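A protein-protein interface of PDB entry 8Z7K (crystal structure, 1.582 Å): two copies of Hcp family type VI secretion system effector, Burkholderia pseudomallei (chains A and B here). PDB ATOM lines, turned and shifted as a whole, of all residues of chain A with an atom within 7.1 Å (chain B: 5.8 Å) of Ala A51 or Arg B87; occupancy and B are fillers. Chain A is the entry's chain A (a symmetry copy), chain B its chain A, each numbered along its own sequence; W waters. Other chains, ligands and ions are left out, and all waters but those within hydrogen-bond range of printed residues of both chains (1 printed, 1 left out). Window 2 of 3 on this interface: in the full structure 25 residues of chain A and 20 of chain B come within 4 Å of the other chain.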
ATOM      1  N   ASP A  48     -18.964  12.330  11.624  1.00  0.00           N
ATOM      2  CA  ASP A  48     -18.045  12.721  10.568  1.00  0.00           C
ATOM      3  C   ASP A  48     -17.404  14.053  10.957  1.00  0.00           C
ATOM      4  O   ASP A  48     -18.093  14.971  11.432  1.00  0.00           O
ATOM      5  CB  ASP A  48     -18.729  12.889   9.221  1.00  0.00           C
ATOM      6  CG  ASP A  48     -17.722  13.243   8.126  1.00  0.00           C
ATOM      7  OD1 ASP A  48     -17.008  12.311   7.700  1.00  0.00           O
ATOM      8  OD2 ASP A  48     -17.519  14.466   7.839  1.00  0.00           O
ATOM      9  N   MET A  49     -16.080  14.138  10.793  1.00  0.00           N
ATOM     10  CA  MET A  49     -15.332  15.355  11.004  1.00  0.00           C
ATOM     11  C   MET A  49     -14.447  15.566   9.777  1.00  0.00           C
ATOM     12  O   MET A  49     -13.608  14.716   9.497  1.00  0.00           O
ATOM     13  CB  MET A  49     -14.469  15.284  12.264  1.00  0.00           C
ATOM     14  CG  MET A  49     -13.578  16.510  12.524  1.00  0.00           C
ATOM     15  SD  MET A  49     -14.483  18.063  12.773  1.00  0.00           S
ATOM     16  CE  MET A  49     -15.067  17.772  14.446  1.00  0.00           C
ATOM     17  N   PRO A  50     -14.563  16.687   9.033  1.00  0.00           N
ATOM     18  CA  PRO A  50     -13.653  16.922   7.901  1.00  0.00           C
ATOM     19  C   PRO A  50     -12.197  17.029   8.373  1.00  0.00           C
ATOM     20  O   PRO A  50     -11.928  17.553   9.449  1.00  0.00           O
ATOM     21  CB  PRO A  50     -14.129  18.256   7.253  1.00  0.00           C
ATOM     22  CG  PRO A  50     -15.406  18.621   7.960  1.00  0.00           C
ATOM     23  CD  PRO A  50     -15.539  17.776   9.221  1.00  0.00           C
ATOM     24  N   ALA A  51     -11.251  16.535   7.569  1.00  0.00           N
ATOM     25  CA  ALA A  51      -9.837  16.610   7.930  1.00  0.00           C
ATOM     26  C   ALA A  51      -9.375  18.069   8.006  1.00  0.00           C
ATOM     27  O   ALA A  51      -8.664  18.442   8.939  1.00  0.00           O
ATOM     28  CB  ALA A  51      -9.011  15.818   6.926  1.00  0.00           C
ATOM     29  N   ARG A  52      -9.828  18.873   7.033  1.00  0.00           N
ATOM     30  CA  ARG A  52      -9.522  20.298   6.954  1.00  0.00           C
ATOM     31  C   ARG A  52     -10.689  21.061   7.566  1.00  0.00           C
ATOM     32  O   ARG A  52     -11.803  20.923   7.063  1.00  0.00           O
ATOM     33  CB  ARG A  52      -9.305  20.749   5.497  1.00  0.00           C
ATOM     34  CG  ARG A  52      -8.749  22.166   5.336  1.00  0.00           C
ATOM     35  CD  ARG A  52      -8.843  22.818   3.934  1.00  0.00           C
ATOM     36  NE  ARG A  52      -9.803  23.927   3.783  1.00  0.00           N
ATOM     37  CZ  ARG A  52      -9.749  25.125   4.386  1.00  0.00           C
ATOM     38  NH1 ARG A  52      -8.760  25.406   5.216  1.00  0.00           N
ATOM     39  NH2 ARG A  52     -10.679  26.047   4.163  1.00  0.00           N
ATOM     40  N   LEU A  53     -10.416  21.818   8.647  1.00  0.00           N
ATOM     41  CA  LEU A  53     -11.400  22.678   9.299  1.00  0.00           C
ATOM     42  C   LEU A  53     -11.379  24.029   8.594  1.00  0.00           C
ATOM     43  O   LEU A  53     -10.317  24.655   8.513  1.00  0.00           O
ATOM     44  CB  LEU A  53     -11.101  22.833  10.783  1.00  0.00           C
ATOM     45  CG  LEU A  53     -12.117  23.595  11.632  1.00  0.00           C
ATOM     46  CD1 LEU A  53     -13.505  22.989  11.504  1.00  0.00           C
ATOM     47  CD2 LEU A  53     -11.688  23.613  13.077  1.00  0.00           C
ATOM     48  N   GLN A  54     -12.533  24.442   8.057  1.00  0.00           N
ATOM     49  CA  GLN A  54     -12.662  25.741   7.412  1.00  0.00           C
ATOM     50  C   GLN A  54     -12.178  26.803   8.398  1.00  0.00           C
ATOM     51  O   GLN A  54     -12.533  26.760   9.577  1.00  0.00           O
ATOM     52  CB  GLN A  54     -14.114  25.950   6.998  1.00  0.00           C
ATOM     53  CG  GLN A  54     -14.479  27.353   6.504  1.00  0.00           C
ATOM     54  CD  GLN A  54     -15.954  27.489   6.182  1.00  0.00           C
ATOM     55  OE1 GLN A  54     -16.678  26.498   6.031  1.00  0.00           O
ATOM     56  NE2 GLN A  54     -16.411  28.721   6.045  1.00  0.00           N
ATOM     57  N   LEU A  57     -14.294  28.238  11.518  1.00  0.00           N
ATOM     58  CA  LEU A  57     -15.467  27.408  11.731  1.00  0.00           C
ATOM     59  C   LEU A  57     -15.298  26.551  12.995  1.00  0.00           C
ATOM     60  O   LEU A  57     -14.250  25.945  13.183  1.00  0.00           O
ATOM     61  CB  LEU A  57     -15.699  26.520  10.517  1.00  0.00           C
ATOM     62  CG  LEU A  57     -17.025  25.754  10.510  1.00  0.00           C
ATOM     63  CD1 LEU A  57     -18.226  26.706  10.508  1.00  0.00           C
ATOM     64  CD2 LEU A  57     -17.063  24.783   9.331  1.00  0.00           C
ATOM     65  N   THR A  58     -16.353  26.470  13.817  1.00  0.00           N
ATOM     66  CA  THR A  58     -16.326  25.612  14.993  1.00  0.00           C
ATOM     67  C   THR A  58     -16.282  24.155  14.554  1.00  0.00           C
ATOM     68  O   THR A  58     -16.928  23.772  13.572  1.00  0.00           O
ATOM     69  CB  THR A  58     -17.514  25.829  15.933  1.00  0.00           C
ATOM     70  OG1 THR A  58     -18.714  25.391  15.288  1.00  0.00           O
ATOM     71  CG2 THR A  58     -17.565  27.265  16.426  1.00  0.00           C
ATOM     72  N   PRO A  59     -15.582  23.284  15.315  1.00  0.00           N
ATOM     73  CA  PRO A  59     -15.704  21.838  15.113  1.00  0.00           C
ATOM     74  C   PRO A  59     -17.142  21.350  14.977  1.00  0.00           C
ATOM     75  O   PRO A  59     -17.456  20.591  14.066  1.00  0.00           O
ATOM     76  CB  PRO A  59     -15.016  21.273  16.353  1.00  0.00           C
ATOM     77  CG  PRO A  59     -13.950  22.296  16.650  1.00  0.00           C
ATOM     78  CD  PRO A  59     -14.618  23.635  16.368  1.00  0.00           C
ATOM     79  N   ALA A  60     -18.024  21.793  15.890  1.00  0.00           N
ATOM     80  CA  ALA A  60     -19.415  21.360  15.893  1.00  0.00           C
ATOM     81  C   ALA A  60     -20.113  21.653  14.566  1.00  0.00           C
ATOM     82  O   ALA A  60     -20.825  20.793  14.025  1.00  0.00           O
ATOM     83  CB  ALA A  60     -20.166  21.994  17.053  1.00  0.00           C
ATOM     84  N   ALA A  62     -18.711  21.971  11.656  1.00  0.00           N
ATOM     85  CA  ALA A  62     -18.077  21.196  10.607  1.00  0.00           C
ATOM     86  C   ALA A  62     -18.536  19.738  10.658  1.00  0.00           C
ATOM     87  O   ALA A  62     -18.591  19.084   9.632  1.00  0.00           O
ATOM     88  CB  ALA A  62     -16.568  21.287  10.729  1.00  0.00           C
ATOM     89  N   GLN B  82     -14.792  11.078  21.819  1.00  0.00           N
ATOM     90  CA  GLN B  82     -14.556  12.454  22.229  1.00  0.00           C
ATOM     91  C   GLN B  82     -13.504  13.154  21.365  1.00  0.00           C
ATOM     92  O   GLN B  82     -13.700  14.317  20.980  1.00  0.00           O
ATOM     93  CB  GLN B  82     -14.111  12.540  23.683  1.00  0.00           C
ATOM     94  CG  GLN B  82     -13.785  13.958  24.119  1.00  0.00           C
ATOM     95  CD  GLN B  82     -13.535  14.041  25.605  1.00  0.00           C
ATOM     96  OE1 GLN B  82     -14.377  13.698  26.431  1.00  0.00           O
ATOM     97  NE2 GLN B  82     -12.373  14.548  25.954  1.00  0.00           N
ATOM     98  N   ALA B  83     -12.348  12.493  21.157  1.00  0.00           N
ATOM     99  CA  ALA B  83     -11.261  13.064  20.368  1.00  0.00           C
ATOM    100  C   ALA B  83     -11.766  13.503  18.994  1.00  0.00           C
ATOM    101  O   ALA B  83     -11.363  14.559  18.500  1.00  0.00           O
ATOM    102  CB  ALA B  83     -10.113  12.064  20.243  1.00  0.00           C
ATOM    103  N   LEU B  84     -12.643  12.681  18.401  1.00  0.00           N
ATOM    104  CA  LEU B  84     -13.234  12.943  17.101  1.00  0.00           C
ATOM    105  C   LEU B  84     -13.937  14.299  17.112  1.00  0.00           C
ATOM    106  O   LEU B  84     -13.673  15.154  16.253  1.00  0.00           O
ATOM    107  CB  LEU B  84     -14.137  11.768  16.703  1.00  0.00           C
ATOM    108  CG  LEU B  84     -15.042  11.954  15.478  1.00  0.00           C
ATOM    109  CD1 LEU B  84     -14.271  12.347  14.217  1.00  0.00           C
ATOM    110  CD2 LEU B  84     -15.860  10.723  15.216  1.00  0.00           C
ATOM    111  N   GLY B  85     -14.823  14.505  18.103  1.00  0.00           N
ATOM    112  CA  GLY B  85     -15.590  15.737  18.146  1.00  0.00           C
ATOM    113  C   GLY B  85     -14.782  16.972  18.550  1.00  0.00           C
ATOM    114  O   GLY B  85     -15.163  18.086  18.200  1.00  0.00           O
ATOM    115  N   LYS B  86     -13.688  16.784  19.292  1.00  0.00           N
ATOM    116  CA  LYS B  86     -12.864  17.878  19.774  1.00  0.00           C
ATOM    117  C   LYS B  86     -11.670  18.148  18.856  1.00  0.00           C
ATOM    118  O   LYS B  86     -10.897  19.046  19.151  1.00  0.00           O
ATOM    119  CB  LYS B  86     -12.403  17.504  21.189  1.00  0.00           C
ATOM    120  CG  LYS B  86     -13.502  17.527  22.235  1.00  0.00           C
ATOM    121  CD  LYS B  86     -12.911  17.660  23.629  1.00  0.00           C
ATOM    122  CE  LYS B  86     -13.862  17.712  24.773  1.00  0.00           C
ATOM    123  NZ  LYS B  86     -14.741  18.877  24.679  1.00  0.00           N
ATOM    124  N   ARG B  87     -11.523  17.402  17.757  1.00  0.00           N
ATOM    125  CA  ARG B  87     -10.343  17.487  16.899  1.00  0.00           C
ATOM    126  C   ARG B  87      -9.042  17.334  17.684  1.00  0.00           C
ATOM    127  O   ARG B  87      -8.064  18.029  17.409  1.00  0.00           O
ATOM    128  CB  ARG B  87     -10.343  18.767  16.057  1.00  0.00           C
ATOM    129  CG  ARG B  87     -11.551  18.900  15.149  1.00  0.00           C
ATOM    130  CD  ARG B  87     -11.431  20.175  14.331  1.00  0.00           C
ATOM    131  NE  ARG B  87     -10.289  20.147  13.405  1.00  0.00           N
ATOM    132  CZ  ARG B  87     -10.257  19.576  12.215  1.00  0.00           C
ATOM    133  NH1 ARG B  87     -11.335  19.011  11.713  1.00  0.00           N
ATOM    134  NH2 ARG B  87      -9.146  19.602  11.487  1.00  0.00           N
ATOM    135  N   GLU B  88      -9.008  16.385  18.617  1.00  0.00           N
ATOM    136  CA  GLU B  88      -7.796  16.135  19.379  1.00  0.00           C
ATOM    137  C   GLU B  88      -6.859  15.295  18.518  1.00  0.00           C
ATOM    138  O   GLU B  88      -7.276  14.246  18.018  1.00  0.00           O
ATOM    139  CB  GLU B  88      -8.129  15.386  20.659  1.00  0.00           C
ATOM    140  CG  GLU B  88      -6.944  15.052  21.554  1.00  0.00           C
ATOM    141  CD  GLU B  88      -7.242  14.041  22.643  1.00  0.00           C
ATOM    142  OE1 GLU B  88      -6.264  13.651  23.328  1.00  0.00           O
ATOM    143  OE2 GLU B  88      -8.418  13.693  22.873  1.00  0.00           O
ATOM    144  N   MET B  89      -5.607  15.747  18.374  1.00  0.00           N
ATOM    145  CA  MET B  89      -4.581  14.997  17.664  1.00  0.00           C
ATOM    146  C   MET B  89      -4.043  13.874  18.546  1.00  0.00           C
ATOM    147  O   MET B  89      -4.006  14.006  19.766  1.00  0.00           O
ATOM    148  CB  MET B  89      -3.466  15.945  17.213  1.00  0.00           C
ATOM    149  CG  MET B  89      -4.005  17.055  16.326  1.00  0.00           C
ATOM    150  SD  MET B  89      -2.774  17.977  15.388  1.00  0.00           S
ATOM    151  CE  MET B  89      -1.704  16.596  14.991  1.00  0.00           C
ATOM    152  N   LEU B 123      -5.458  12.628  13.040  1.00  0.00           N
ATOM    153  CA  LEU B 123      -6.751  13.140  13.447  1.00  0.00           C
ATOM    154  C   LEU B 123      -7.808  12.097  13.120  1.00  0.00           C
ATOM    155  O   LEU B 123      -7.812  11.524  12.041  1.00  0.00           O
ATOM    156  CB  LEU B 123      -7.001  14.421  12.661  1.00  0.00           C
ATOM    157  CG  LEU B 123      -8.226  15.240  13.072  1.00  0.00           C
ATOM    158  CD1 LEU B 123      -7.937  15.999  14.342  1.00  0.00           C
ATOM    159  CD2 LEU B 123      -8.623  16.196  11.955  1.00  0.00           C
ATOM    160  N   THR B 125     -11.294  11.214  11.776  1.00  0.00           N
ATOM    161  CA  THR B 125     -12.171  11.898  10.839  1.00  0.00           C
ATOM    162  C   THR B 125     -13.507  11.208  10.674  1.00  0.00           C
ATOM    163  O   THR B 125     -14.427  11.826  10.133  1.00  0.00           O
ATOM    164  CB  THR B 125     -11.439  12.105   9.510  1.00  0.00           C
ATOM    165  OG1 THR B 125     -10.900  10.873   9.042  1.00  0.00           O
ATOM    166  CG2 THR B 125     -10.311  13.111   9.660  1.00  0.00           C
ATOM    167  N   THR B 156      -7.052  10.221   9.656  1.00  0.00           N
ATOM    168  CA  THR B 156      -6.299  10.838   8.600  1.00  0.00           C
ATOM    169  C   THR B 156      -4.947  11.220   9.189  1.00  0.00           C
ATOM    170  O   THR B 156      -4.859  11.606  10.352  1.00  0.00           O
ATOM    171  CB  THR B 156      -7.082  12.048   8.072  1.00  0.00           C
ATOM    172  OG1 THR B 156      -8.329  11.557   7.570  1.00  0.00           O
ATOM    173  CG2 THR B 156      -6.344  12.747   6.947  1.00  0.00           C
HETATM  174  O   HOH W   1     -17.510  18.685  16.821  1.00  0.00           O
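The side-chain sulfur (SD) of Met A49 lies within hydrogen-bond range of the guanidinium group (NH1) of Arg B87 (3.5 Å). O of Pro A50 sits at hydrogen-bond distance from NH1 of Arg B87, at 2.8 Å. NH2 of Arg B87 is in hydrogen-bond range of O of Ala A51 (2.8 Å). The backbone carbonyl oxygen (O) of Thr B125 sits at hydrogen-bond distance from the backbone NH (N) of Met A49 (2.9 Å).
N of Thr B156 is in hydrogen-bond range of O of Leu B123 (2.8 Å). The side-chain hydroxyl (OG1) of Thr B125 sits at hydrogen-bond distance from the side-chain hydroxyl (OG1) of Thr B156, at 3.0 Å.
Among the printed residues, merely in contact across the chains: Met A49 with Leu B84 (3.5 Å), Asp A48 with Thr B125 (3.6 Å), Leu A53 with Arg B87 (3.7 Å), Pro A59 with Gly B85 (3.7 Å), Ala A51 with Leu B123 (3.8 Å), Met A49 with Gly B85 (3.8 Å) and Ala A51 with Thr B125 (3.9 Å).
Of chain B, only Arg B87, Leu B123 and Thr B125 come within 4 Å of Ala A51. Of chain A, only Met A49, Pro A50, Ala A51 and Leu A53 come within 4 Å of Arg B87. Of the printed residues of chain A, Leu B123 touches Ala A51 (3.8 Å). Of the printed residues of chain B, Pro A59 touches Gly B85 (3.7 Å). Of the printed residues of chain B, Leu A53 touches Arg B87 (3.7 Å). Gln B82 touches none of the printed residues of chain A. The nearest printed residue of chain B that does not touch Asp A48 is Leu B84 (4.8 Å).
Hydrophobic or aromatic side chains of chain B that line the printed part of chain A: Leu B84 and Leu B123. Printed residues of chain A that touch a printed residue of chain B: Asp A48, Met A49, Pro A50, Ala A51, Leu A53 and Pro A59. Hydrophobic or aromatic side chains of chain A within 4 Å of the printed part of chain B: Met A49, Leu A53 and Pro A59. Among the printed residues, 11 pairs touch across the chains.
No position is printed for both chains.
Water W1 lies within hydrogen-bond range of the backbone carbonyl oxygen of Gly B85, the backbone NH of Ala A60 and the backbone carbonyl oxygen of Pro A59.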
